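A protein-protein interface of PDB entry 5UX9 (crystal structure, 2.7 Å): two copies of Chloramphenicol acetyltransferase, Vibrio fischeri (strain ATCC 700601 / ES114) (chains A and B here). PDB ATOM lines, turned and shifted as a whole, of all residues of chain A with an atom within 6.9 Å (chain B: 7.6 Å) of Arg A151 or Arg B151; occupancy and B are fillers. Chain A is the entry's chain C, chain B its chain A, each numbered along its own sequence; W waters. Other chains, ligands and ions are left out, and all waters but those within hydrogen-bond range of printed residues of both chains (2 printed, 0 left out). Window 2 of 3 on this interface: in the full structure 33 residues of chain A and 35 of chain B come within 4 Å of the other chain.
Glu A133 touches Arg B151, but with the chains exchanged Arg A151 does not touch Glu B133 (7.3 Å).
Ala A134 touches Arg B151, but with the chains exchanged Arg A151 does not touch Ala B134 (11.0 Å).
Met A135 touches Ala B150, but with the chains exchanged Ala A150 does not touch Met B135 (15.1 Å).
Met A135 touches Arg B151, but with the chains exchanged Arg A151 does not touch Met B135 (8.5 Å).
Of the 8 pairs that touch across the chains among the printed residues, 1 has its exchanged pair printed and touching as well.
Water W2 lies within hydrogen-bond range of the side-chain amide oxygen of Asn A167 (2.8 Å) and the backbone NH of Asn B167 (3.2 Å).
Water W1 bridges the side-chain hydroxyl (OG) of Ser B132 and the guanidinium group (NH1) of Arg A48.
The backbone carbonyl oxygen (O) of Glu A133 sits at hydrogen-bond distance from the guanidinium group (NH1) of Arg B151 (2.5 Å).
The guanidinium group of Arg A48 lies within salt-bridge range of the side-chain carboxylate of Glu B133 (2.8 Å).
Of the 20 printed residues of chain B, 4 touch a printed residue of chain A.
Along chain B the printed residues that touch a printed residue of chain A span positions 133 to 166.
Of the 19 printed residues of chain A, 7 touch a printed residue of chain B.
Printed residues of chain A that touch a printed residue of chain B: Arg A48, Glu A133, Ala A134, Met A135, Met A137, Arg A151 and Asn A167.
Among the printed residues, 8 pairs touch across the chains.
Among the printed residues, Asp or Glu carboxylates within 4 Å of a Lys or Arg side-chain nitrogen of the other chain: Arg A48 with Glu B133 (2.8 Å).
Ala A134 touches Arg B151.
Ala B150 touches Met A135.
Met A135 touches Arg B151.
Ala B150 touches Met A137 (CB to CE, 3.8 Å).
Arg B151 touches Arg A151 (NH1 to O, 3.9 Å).
Asn A167 touches Gly B166.
Of chain B, only Arg B151 (3.9 Å) comes within 4 Å of Arg A151.
Of chain A, only Glu A133 (2.5 Å), Ala A134 (3.97 Å), Met A135 (3.8 Å) and Arg A151 (3.9 Å) come within 4 Å of Arg B151.
Of the printed residues of chain B, Ala A134 touches Arg B151 (3.97 Å).
Of the printed residues of chain B, Asn A167 touches Gly B166.
Of the printed residues of chain A, Ala B150 touches Met A135 (3.7 Å) and Met A137 (3.8 Å).
Of the printed residues of chain A, Glu B133 touches Arg A48 (2.8 Å).
Of the printed residues of chain B, Met A137 touches Ala B150 (3.8 Å).
Val B164 touches none of the printed residues of chain A.
Val B153 touches none of the printed residues of chain A.
The nearest residue of chain A that does not touch Arg B151 is Ala A152 (4.1 Å).
The backbone NH of Glu B133 sits at hydrogen-bond distance from the backbone carbonyl oxygen of Ser B81 (3.0 Å).
The backbone carbonyl oxygen of Ser B132 is in hydrogen-bond range of the backbone NH of Arg B151 (2.8 Å).
NE of Arg A151 lies within salt-bridge range of OE1 of Glu A133.
The backbone NH (N) of Met A135 is in hydrogen-bond range of the backbone carbonyl oxygen (O) of Ala A152, at 2.8 Å.
OE2 of Glu B133 is in salt-bridge range of NE of Arg B151, at 3.2 Å.
N of Thr A84 sits at hydrogen-bond distance from O of Ala A134 (2.7 Å).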
ATOM      1  N   ARG A  48      20.625  28.696 -10.131  1.00  0.00           N
ATOM      2  CA  ARG A  48      21.944  28.761 -10.741  1.00  0.00           C
ATOM      3  C   ARG A  48      21.991  29.865 -11.787  1.00  0.00           C
ATOM      4  O   ARG A  48      21.033  30.061 -12.540  1.00  0.00           O
ATOM      5  CB  ARG A  48      22.321  27.419 -11.372  1.00  0.00           C
ATOM      6  CG  ARG A  48      22.315  26.273 -10.379  1.00  0.00           C
ATOM      7  CD  ARG A  48      22.925  25.006 -10.950  1.00  0.00           C
ATOM      8  NE  ARG A  48      22.948  23.939  -9.952  1.00  0.00           N
ATOM      9  CZ  ARG A  48      23.395  22.707 -10.177  1.00  0.00           C
ATOM     10  NH1 ARG A  48      23.858  22.375 -11.373  1.00  0.00           N
ATOM     11  NH2 ARG A  48      23.376  21.808  -9.202  1.00  0.00           N
ATOM     12  N   GLY A  82      17.872  18.676  -4.794  1.00  0.00           N
ATOM     13  CA  GLY A  82      18.561  18.664  -6.066  1.00  0.00           C
ATOM     14  C   GLY A  82      17.819  19.298  -7.219  1.00  0.00           C
ATOM     15  O   GLY A  82      18.380  19.378  -8.320  1.00  0.00           O
ATOM     16  N   ALA A  83      16.577  19.736  -7.017  1.00  0.00           N
ATOM     17  CA  ALA A  83      15.870  20.457  -8.064  1.00  0.00           C
ATOM     18  C   ALA A  83      16.639  21.719  -8.435  1.00  0.00           C
ATOM     19  O   ALA A  83      17.274  22.358  -7.591  1.00  0.00           O
ATOM     20  CB  ALA A  83      14.453  20.806  -7.612  1.00  0.00           C
ATOM     21  N   THR A  84      16.589  22.074  -9.716  1.00  0.00           N
ATOM     22  CA  THR A  84      17.448  23.121 -10.249  1.00  0.00           C
ATOM     23  C   THR A  84      16.648  24.053 -11.143  1.00  0.00           C
ATOM     24  O   THR A  84      15.815  23.604 -11.936  1.00  0.00           O
ATOM     25  CB  THR A  84      18.619  22.520 -11.038  1.00  0.00           C
ATOM     26  OG1 THR A  84      19.234  21.485 -10.261  1.00  0.00           O
ATOM     27  CG2 THR A  84      19.652  23.584 -11.352  1.00  0.00           C
ATOM     28  N   GLY A 131       9.973  17.327  -8.290  1.00  0.00           N
ATOM     29  CA  GLY A 131      10.674  16.146  -7.827  1.00  0.00           C
ATOM     30  C   GLY A 131      12.165  16.372  -7.656  1.00  0.00           C
ATOM     31  O   GLY A 131      12.728  17.420  -7.972  1.00  0.00           O
ATOM     32  N   SER A 132      12.815  15.333  -7.140  1.00  0.00           N
ATOM     33  CA  SER A 132      14.226  15.420  -6.798  1.00  0.00           C
ATOM     34  C   SER A 132      15.096  15.460  -8.047  1.00  0.00           C
ATOM     35  O   SER A 132      14.887  14.700  -8.997  1.00  0.00           O
ATOM     36  CB  SER A 132      14.630  14.238  -5.920  1.00  0.00           C
ATOM     37  OG  SER A 132      16.013  14.281  -5.616  1.00  0.00           O
ATOM     38  N   GLU A 133      16.083  16.359  -8.033  1.00  0.00           N
ATOM     39  CA  GLU A 133      17.073  16.488  -9.103  1.00  0.00           C
ATOM     40  C   GLU A 133      16.425  16.760 -10.458  1.00  0.00           C
ATOM     41  O   GLU A 133      16.936  16.341 -11.496  1.00  0.00           O
ATOM     42  CB  GLU A 133      17.980  15.256  -9.175  1.00  0.00           C
ATOM     43  CG  GLU A 133      18.848  15.063  -7.940  1.00  0.00           C
ATOM     44  CD  GLU A 133      19.845  13.932  -8.093  1.00  0.00           C
ATOM     45  OE1 GLU A 133      20.354  13.734  -9.217  1.00  0.00           O
ATOM     46  OE2 GLU A 133      20.122  13.241  -7.089  1.00  0.00           O
ATOM     47  N   ALA A 134      15.292  17.453 -10.458  1.00  0.00           N
ATOM     48  CA  ALA A 134      14.714  17.939 -11.698  1.00  0.00           C
ATOM     49  C   ALA A 134      15.354  19.270 -12.068  1.00  0.00           C
ATOM     50  O   ALA A 134      15.883  19.986 -11.215  1.00  0.00           O
ATOM     51  CB  ALA A 134      13.200  18.098 -11.568  1.00  0.00           C
ATOM     52  N   MET A 135      15.312  19.597 -13.350  1.00  0.00           N
ATOM     53  CA  MET A 135      15.985  20.786 -13.843  1.00  0.00           C
ATOM     54  C   MET A 135      15.066  21.578 -14.766  1.00  0.00           C
ATOM     55  O   MET A 135      14.552  21.052 -15.752  1.00  0.00           O
ATOM     56  CB  MET A 135      17.290  20.395 -14.545  1.00  0.00           C
ATOM     57  CG  MET A 135      17.819  21.420 -15.536  1.00  0.00           C
ATOM     58  SD  MET A 135      19.007  20.670 -16.894  1.00  0.00           S
ATOM     59  CE  MET A 135      20.740  21.208 -16.195  1.00  0.00           C
ATOM     60  N   MET A 137      14.534  24.668 -17.314  1.00  0.00           N
ATOM     61  CA  MET A 137      15.253  25.568 -18.219  1.00  0.00           C
ATOM     62  C   MET A 137      14.701  27.003 -18.179  1.00  0.00           C
ATOM     63  O   MET A 137      13.582  27.217 -17.712  1.00  0.00           O
ATOM     64  CB  MET A 137      15.210  25.012 -19.645  1.00  0.00           C
ATOM     65  CG  MET A 137      15.599  23.548 -19.754  1.00  0.00           C
ATOM     66  SD  MET A 137      17.008  22.994 -18.506  1.00  0.00           S
ATOM     67  CE  MET A 137      18.580  23.719 -19.392  1.00  0.00           C
ATOM     68  N   ILE A 148       6.111  17.910 -11.231  1.00  0.00           N
ATOM     69  CA  ILE A 148       7.295  17.639 -12.037  1.00  0.00           C
ATOM     70  C   ILE A 148       7.979  16.414 -11.450  1.00  0.00           C
ATOM     71  O   ILE A 148       8.363  16.414 -10.273  1.00  0.00           O
ATOM     72  CB  ILE A 148       8.251  18.841 -12.072  1.00  0.00           C
ATOM     73  CG1 ILE A 148       7.516  20.096 -12.551  1.00  0.00           C
ATOM     74  CG2 ILE A 148       9.450  18.542 -12.959  1.00  0.00           C
ATOM     75  CD1 ILE A 148       6.897  19.956 -13.927  1.00  0.00           C
ATOM     76  N   GLY A 149       8.125  15.371 -12.265  1.00  0.00           N
ATOM     77  CA  GLY A 149       8.748  14.153 -11.797  1.00  0.00           C
ATOM     78  C   GLY A 149      10.215  14.338 -11.466  1.00  0.00           C
ATOM     79  O   GLY A 149      10.853  15.325 -11.835  1.00  0.00           O
ATOM     80  N   ALA A 150      10.756  13.363 -10.742  1.00  0.00           N
ATOM     81  CA  ALA A 150      12.163  13.402 -10.370  1.00  0.00           C
ATOM     82  C   ALA A 150      13.043  13.229 -11.601  1.00  0.00           C
ATOM     83  O   ALA A 150      12.699  12.497 -12.535  1.00  0.00           O
ATOM     84  CB  ALA A 150      12.472  12.315  -9.341  1.00  0.00           C
ATOM     85  N   ARG A 151      14.180  13.927 -11.604  1.00  0.00           N
ATOM     86  CA  ARG A 151      15.155  13.900 -12.695  1.00  0.00           C
ATOM     87  C   ARG A 151      14.562  14.366 -14.022  1.00  0.00           C
ATOM     88  O   ARG A 151      15.137  14.113 -15.085  1.00  0.00           O
ATOM     89  CB  ARG A 151      15.775  12.508 -12.859  1.00  0.00           C
ATOM     90  CG  ARG A 151      16.819  12.165 -11.810  1.00  0.00           C
ATOM     91  CD  ARG A 151      18.203  12.641 -12.220  1.00  0.00           C
ATOM     92  NE  ARG A 151      19.225  12.185 -11.284  1.00  0.00           N
ATOM     93  CZ  ARG A 151      19.836  11.006 -11.354  1.00  0.00           C
ATOM     94  NH1 ARG A 151      19.533  10.156 -12.326  1.00  0.00           N
ATOM     95  NH2 ARG A 151      20.751  10.678 -10.453  1.00  0.00           N
ATOM     96  N   ALA A 152      13.422  15.051 -13.985  1.00  0.00           N
ATOM     97  CA  ALA A 152      12.800  15.539 -15.205  1.00  0.00           C
ATOM     98  C   ALA A 152      13.486  16.812 -15.685  1.00  0.00           C
ATOM     99  O   ALA A 152      13.960  17.628 -14.891  1.00  0.00           O
ATOM    100  CB  ALA A 152      11.310  15.803 -14.984  1.00  0.00           C
ATOM    101  N   VAL A 153      13.541  16.972 -17.003  1.00  0.00           N
ATOM    102  CA  VAL A 153      14.094  18.164 -17.633  1.00  0.00           C
ATOM    103  C   VAL A 153      12.943  18.884 -18.321  1.00  0.00           C
ATOM    104  O   VAL A 153      12.388  18.388 -19.310  1.00  0.00           O
ATOM    105  CB  VAL A 153      15.218  17.824 -18.621  1.00  0.00           C
ATOM    106  CG1 VAL A 153      15.802  19.098 -19.213  1.00  0.00           C
ATOM    107  CG2 VAL A 153      16.300  17.015 -17.928  1.00  0.00           C
ATOM    108  N   VAL A 165       6.920  14.065 -16.606  1.00  0.00           N
ATOM    109  CA  VAL A 165       8.040  13.221 -16.219  1.00  0.00           C
ATOM    110  C   VAL A 165       9.060  13.201 -17.347  1.00  0.00           C
ATOM    111  O   VAL A 165       8.777  13.585 -18.485  1.00  0.00           O
ATOM    112  CB  VAL A 165       7.604  11.777 -15.879  1.00  0.00           C
ATOM    113  CG1 VAL A 165       6.407  11.782 -14.942  1.00  0.00           C
ATOM    114  CG2 VAL A 165       7.298  10.998 -17.152  1.00  0.00           C
ATOM    115  N   GLY A 166      10.261  12.739 -17.010  1.00  0.00           N
ATOM    116  CA  GLY A 166      11.298  12.543 -18.006  1.00  0.00           C
ATOM    117  C   GLY A 166      11.630  13.824 -18.737  1.00  0.00           C
ATOM    118  O   GLY A 166      11.652  14.917 -18.160  1.00  0.00           O
ATOM    119  N   ASN A 167      11.890  13.696 -20.035  1.00  0.00           N
ATOM    120  CA  ASN A 167      12.233  14.848 -20.862  1.00  0.00           C
ATOM    121  C   ASN A 167      10.946  15.505 -21.355  1.00  0.00           C
ATOM    122  O   ASN A 167      10.576  15.453 -22.528  1.00  0.00           O
ATOM    123  CB  ASN A 167      13.152  14.429 -21.999  1.00  0.00           C
ATOM    124  CG  ASN A 167      14.475  13.904 -21.493  1.00  0.00           C
ATOM    125  OD1 ASN A 167      15.034  12.957 -22.043  1.00  0.00           O
ATOM    126  ND2 ASN A 167      14.979  14.511 -20.423  1.00  0.00           N
ATOM    127  N   SER B  81      29.139  23.517 -16.252  1.00  0.00           N
ATOM    128  CA  SER B  81      29.406  22.832 -14.995  1.00  0.00           C
ATOM    129  C   SER B  81      28.635  21.519 -14.920  1.00  0.00           C
ATOM    130  O   SER B  81      27.422  21.479 -15.153  1.00  0.00           O
ATOM    131  CB  SER B  81      29.039  23.741 -13.819  1.00  0.00           C
ATOM    132  OG  SER B  81      29.214  23.095 -12.569  1.00  0.00           O
ATOM    133  N   GLY B  82      29.368  20.473 -14.537  1.00  0.00           N
ATOM    134  CA  GLY B  82      28.811  19.148 -14.407  1.00  0.00           C
ATOM    135  C   GLY B  82      28.940  18.270 -15.630  1.00  0.00           C
ATOM    136  O   GLY B  82      28.644  17.070 -15.542  1.00  0.00           O
ATOM    137  N   ALA B  83      29.351  18.825 -16.769  1.00  0.00           N
ATOM    138  CA  ALA B  83      29.583  18.014 -17.957  1.00  0.00           C
ATOM    139  C   ALA B  83      30.657  16.974 -17.668  1.00  0.00           C
ATOM    140  O   ALA B  83      31.782  17.318 -17.294  1.00  0.00           O
ATOM    141  CB  ALA B  83      29.993  18.902 -19.131  1.00  0.00           C
ATOM    142  N   ILE B 130      29.027  22.163 -24.752  1.00  0.00           N
ATOM    143  CA  ILE B 130      28.463  21.027 -24.031  1.00  0.00           C
ATOM    144  C   ILE B 130      27.733  21.574 -22.813  1.00  0.00           C
ATOM    145  O   ILE B 130      28.349  22.198 -21.940  1.00  0.00           O
ATOM    146  CB  ILE B 130      29.550  20.015 -23.632  1.00  0.00           C
ATOM    147  CG1 ILE B 130      30.383  19.611 -24.853  1.00  0.00           C
ATOM    148  CG2 ILE B 130      28.938  18.787 -22.953  1.00  0.00           C
ATOM    149  CD1 ILE B 130      31.353  18.480 -24.579  1.00  0.00           C
ATOM    150  N   GLY B 131      26.415  21.357 -22.768  1.00  0.00           N
ATOM    151  CA  GLY B 131      25.590  21.898 -21.706  1.00  0.00           C
ATOM    152  C   GLY B 131      25.916  21.330 -20.336  1.00  0.00           C
ATOM    153  O   GLY B 131      26.683  20.380 -20.181  1.00  0.00           O
ATOM    154  N   SER B 132      25.304  21.936 -19.320  1.00  0.00           N
ATOM    155  CA  SER B 132      25.601  21.586 -17.936  1.00  0.00           C
ATOM    156  C   SER B 132      25.113  20.181 -17.598  1.00  0.00           C
ATOM    157  O   SER B 132      24.016  19.774 -17.990  1.00  0.00           O
ATOM    158  CB  SER B 132      24.961  22.599 -16.989  1.00  0.00           C
ATOM    159  OG  SER B 132      25.140  22.225 -15.632  1.00  0.00           O
ATOM    160  N   GLU B 133      25.948  19.442 -16.861  1.00  0.00           N
ATOM    161  CA  GLU B 133      25.611  18.117 -16.338  1.00  0.00           C
ATOM    162  C   GLU B 133      25.287  17.119 -17.448  1.00  0.00           C
ATOM    163  O   GLU B 133      24.552  16.154 -17.231  1.00  0.00           O
ATOM    164  CB  GLU B 133      24.464  18.195 -15.327  1.00  0.00           C
ATOM    165  CG  GLU B 133      24.915  18.643 -13.944  1.00  0.00           C
ATOM    166  CD  GLU B 133      23.761  18.901 -13.000  1.00  0.00           C
ATOM    167  OE1 GLU B 133      23.935  19.696 -12.050  1.00  0.00           O
ATOM    168  OE2 GLU B 133      22.680  18.309 -13.204  1.00  0.00           O
ATOM    169  N   ALA B 134      25.840  17.334 -18.638  1.00  0.00           N
ATOM    170  CA  ALA B 134      25.724  16.358 -19.709  1.00  0.00           C
ATOM    171  C   ALA B 134      26.765  15.259 -19.531  1.00  0.00           C
ATOM    172  O   ALA B 134      27.829  15.472 -18.942  1.00  0.00           O
ATOM    173  CB  ALA B 134      25.896  17.026 -21.072  1.00  0.00           C
ATOM    174  N   MET B 135      26.448  14.075 -20.041  1.00  0.00           N
ATOM    175  CA  MET B 135      27.350  12.938 -19.893  1.00  0.00           C
ATOM    176  C   MET B 135      27.757  12.362 -21.248  1.00  0.00           C
ATOM    177  O   MET B 135      26.907  12.018 -22.070  1.00  0.00           O
ATOM    178  CB  MET B 135      26.704  11.853 -19.030  1.00  0.00           C
ATOM    179  CG  MET B 135      27.601  10.648 -18.799  1.00  0.00           C
ATOM    180  SD  MET B 135      26.680   9.138 -17.985  1.00  0.00           S
ATOM    181  CE  MET B 135      27.078   9.494 -16.118  1.00  0.00           C
ATOM    182  N   ILE B 148      25.718  20.250 -27.397  1.00  0.00           N
ATOM    183  CA  ILE B 148      25.147  19.219 -26.541  1.00  0.00           C
ATOM    184  C   ILE B 148      24.278  19.904 -25.497  1.00  0.00           C
ATOM    185  O   ILE B 148      24.729  20.834 -24.817  1.00  0.00           O
ATOM    186  CB  ILE B 148      26.241  18.364 -25.879  1.00  0.00           C
ATOM    187  CG1 ILE B 148      27.211  17.828 -26.933  1.00  0.00           C
ATOM    188  CG2 ILE B 148      25.621  17.219 -25.098  1.00  0.00           C
ATOM    189  CD1 ILE B 148      26.566  16.900 -27.943  1.00  0.00           C
ATOM    190  N   GLY B 149      23.033  19.453 -25.376  1.00  0.00           N
ATOM    191  CA  GLY B 149      22.115  20.047 -24.428  1.00  0.00           C
ATOM    192  C   GLY B 149      22.445  19.677 -22.996  1.00  0.00           C
ATOM    193  O   GLY B 149      23.224  18.766 -22.708  1.00  0.00           O
ATOM    194  N   ALA B 150      21.828  20.411 -22.073  1.00  0.00           N
ATOM    195  CA  ALA B 150      22.048  20.169 -20.655  1.00  0.00           C
ATOM    196  C   ALA B 150      21.471  18.820 -20.244  1.00  0.00           C
ATOM    197  O   ALA B 150      20.364  18.450 -20.644  1.00  0.00           O
ATOM    198  CB  ALA B 150      21.423  21.287 -19.820  1.00  0.00           C
ATOM    199  N   ARG B 151      22.242  18.082 -19.442  1.00  0.00           N
ATOM    200  CA  ARG B 151      21.856  16.765 -18.929  1.00  0.00           C
ATOM    201  C   ARG B 151      21.583  15.767 -20.049  1.00  0.00           C
ATOM    202  O   ARG B 151      20.835  14.801 -19.866  1.00  0.00           O
ATOM    203  CB  ARG B 151      20.651  16.858 -17.991  1.00  0.00           C
ATOM    204  CG  ARG B 151      21.044  16.910 -16.528  1.00  0.00           C
ATOM    205  CD  ARG B 151      19.914  16.457 -15.635  1.00  0.00           C
ATOM    206  NE  ARG B 151      19.992  17.083 -14.320  1.00  0.00           N
ATOM    207  CZ  ARG B 151      18.982  17.130 -13.460  1.00  0.00           C
ATOM    208  NH1 ARG B 151      17.814  16.586 -13.776  1.00  0.00           N
ATOM    209  NH2 ARG B 151      19.138  17.721 -12.283  1.00  0.00           N
ATOM    210  N   ALA B 152      22.188  15.987 -21.209  1.00  0.00           N
ATOM    211  CA  ALA B 152      22.106  15.028 -22.296  1.00  0.00           C
ATOM    212  C   ALA B 152      23.104  13.900 -22.077  1.00  0.00           C
ATOM    213  O   ALA B 152      24.181  14.096 -21.505  1.00  0.00           O
ATOM    214  CB  ALA B 152      22.371  15.707 -23.639  1.00  0.00           C
ATOM    215  N   VAL B 153      22.735  12.708 -22.530  1.00  0.00           N
ATOM    216  CA  VAL B 153      23.598  11.536 -22.454  1.00  0.00           C
ATOM    217  C   VAL B 153      23.949  11.137 -23.881  1.00  0.00           C
ATOM    218  O   VAL B 153      23.108  10.598 -24.612  1.00  0.00           O
ATOM    219  CB  VAL B 153      22.933  10.383 -21.691  1.00  0.00           C
ATOM    220  CG1 VAL B 153      23.896   9.213 -21.557  1.00  0.00           C
ATOM    221  CG2 VAL B 153      22.472  10.856 -20.320  1.00  0.00           C
ATOM    222  N   ILE B 154      25.190  11.404 -24.276  1.00  0.00           N
ATOM    223  CA  ILE B 154      25.665  11.133 -25.629  1.00  0.00           C
ATOM    224  C   ILE B 154      26.339   9.765 -25.631  1.00  0.00           C
ATOM    225  O   ILE B 154      27.369   9.565 -24.981  1.00  0.00           O
ATOM    226  CB  ILE B 154      26.623  12.227 -26.117  1.00  0.00           C
ATOM    227  CG1 ILE B 154      25.974  13.612 -26.004  1.00  0.00           C
ATOM    228  CG2 ILE B 154      27.070  11.956 -27.543  1.00  0.00           C
ATOM    229  CD1 ILE B 154      24.607  13.719 -26.651  1.00  0.00           C
ATOM    230  N   VAL B 164      22.120  18.158 -30.150  1.00  0.00           N
ATOM    231  CA  VAL B 164      21.687  16.900 -29.552  1.00  0.00           C
ATOM    232  C   VAL B 164      21.256  17.174 -28.118  1.00  0.00           C
ATOM    233  O   VAL B 164      22.049  17.673 -27.310  1.00  0.00           O
ATOM    234  CB  VAL B 164      22.796  15.837 -29.592  1.00  0.00           C
ATOM    235  CG1 VAL B 164      22.214  14.458 -29.315  1.00  0.00           C
ATOM    236  CG2 VAL B 164      23.511  15.863 -30.933  1.00  0.00           C
ATOM    237  N   VAL B 165      20.004  16.846 -27.804  1.00  0.00           N
ATOM    238  CA  VAL B 165      19.456  17.005 -26.465  1.00  0.00           C
ATOM    239  C   VAL B 165      18.939  15.651 -25.989  1.00  0.00           C
ATOM    240  O   VAL B 165      18.783  14.710 -26.768  1.00  0.00           O
ATOM    241  CB  VAL B 165      18.338  18.066 -26.412  1.00  0.00           C
ATOM    242  CG1 VAL B 165      18.770  19.339 -27.127  1.00  0.00           C
ATOM    243  CG2 VAL B 165      17.054  17.516 -27.012  1.00  0.00           C
ATOM    244  N   GLY B 166      18.676  15.566 -24.687  1.00  0.00           N
ATOM    245  CA  GLY B 166      18.105  14.349 -24.133  1.00  0.00           C
ATOM    246  C   GLY B 166      19.035  13.164 -24.283  1.00  0.00           C
ATOM    247  O   GLY B 166      20.260  13.283 -24.182  1.00  0.00           O
ATOM    248  N   ASN B 167      18.450  11.994 -24.536  1.00  0.00           N
ATOM    249  CA  ASN B 167      19.225  10.763 -24.689  1.00  0.00           C
ATOM    250  C   ASN B 167      19.518  10.550 -26.172  1.00  0.00           C
ATOM    251  O   ASN B 167      18.889   9.742 -26.858  1.00  0.00           O
ATOM    252  CB  ASN B 167      18.484   9.582 -24.076  1.00  0.00           C
ATOM    253  CG  ASN B 167      18.211   9.772 -22.594  1.00  0.00           C
ATOM    254  OD1 ASN B 167      18.952  10.468 -21.897  1.00  0.00           O
ATOM    255  ND2 ASN B 167      17.143   9.150 -22.104  1.00  0.00           N
HETATM  256  O   HOH W   1      24.754  24.185 -13.585  1.00  0.00           O
HETATM  257  O   HOH W   2      15.294  11.649 -24.517  1.00  0.00           O
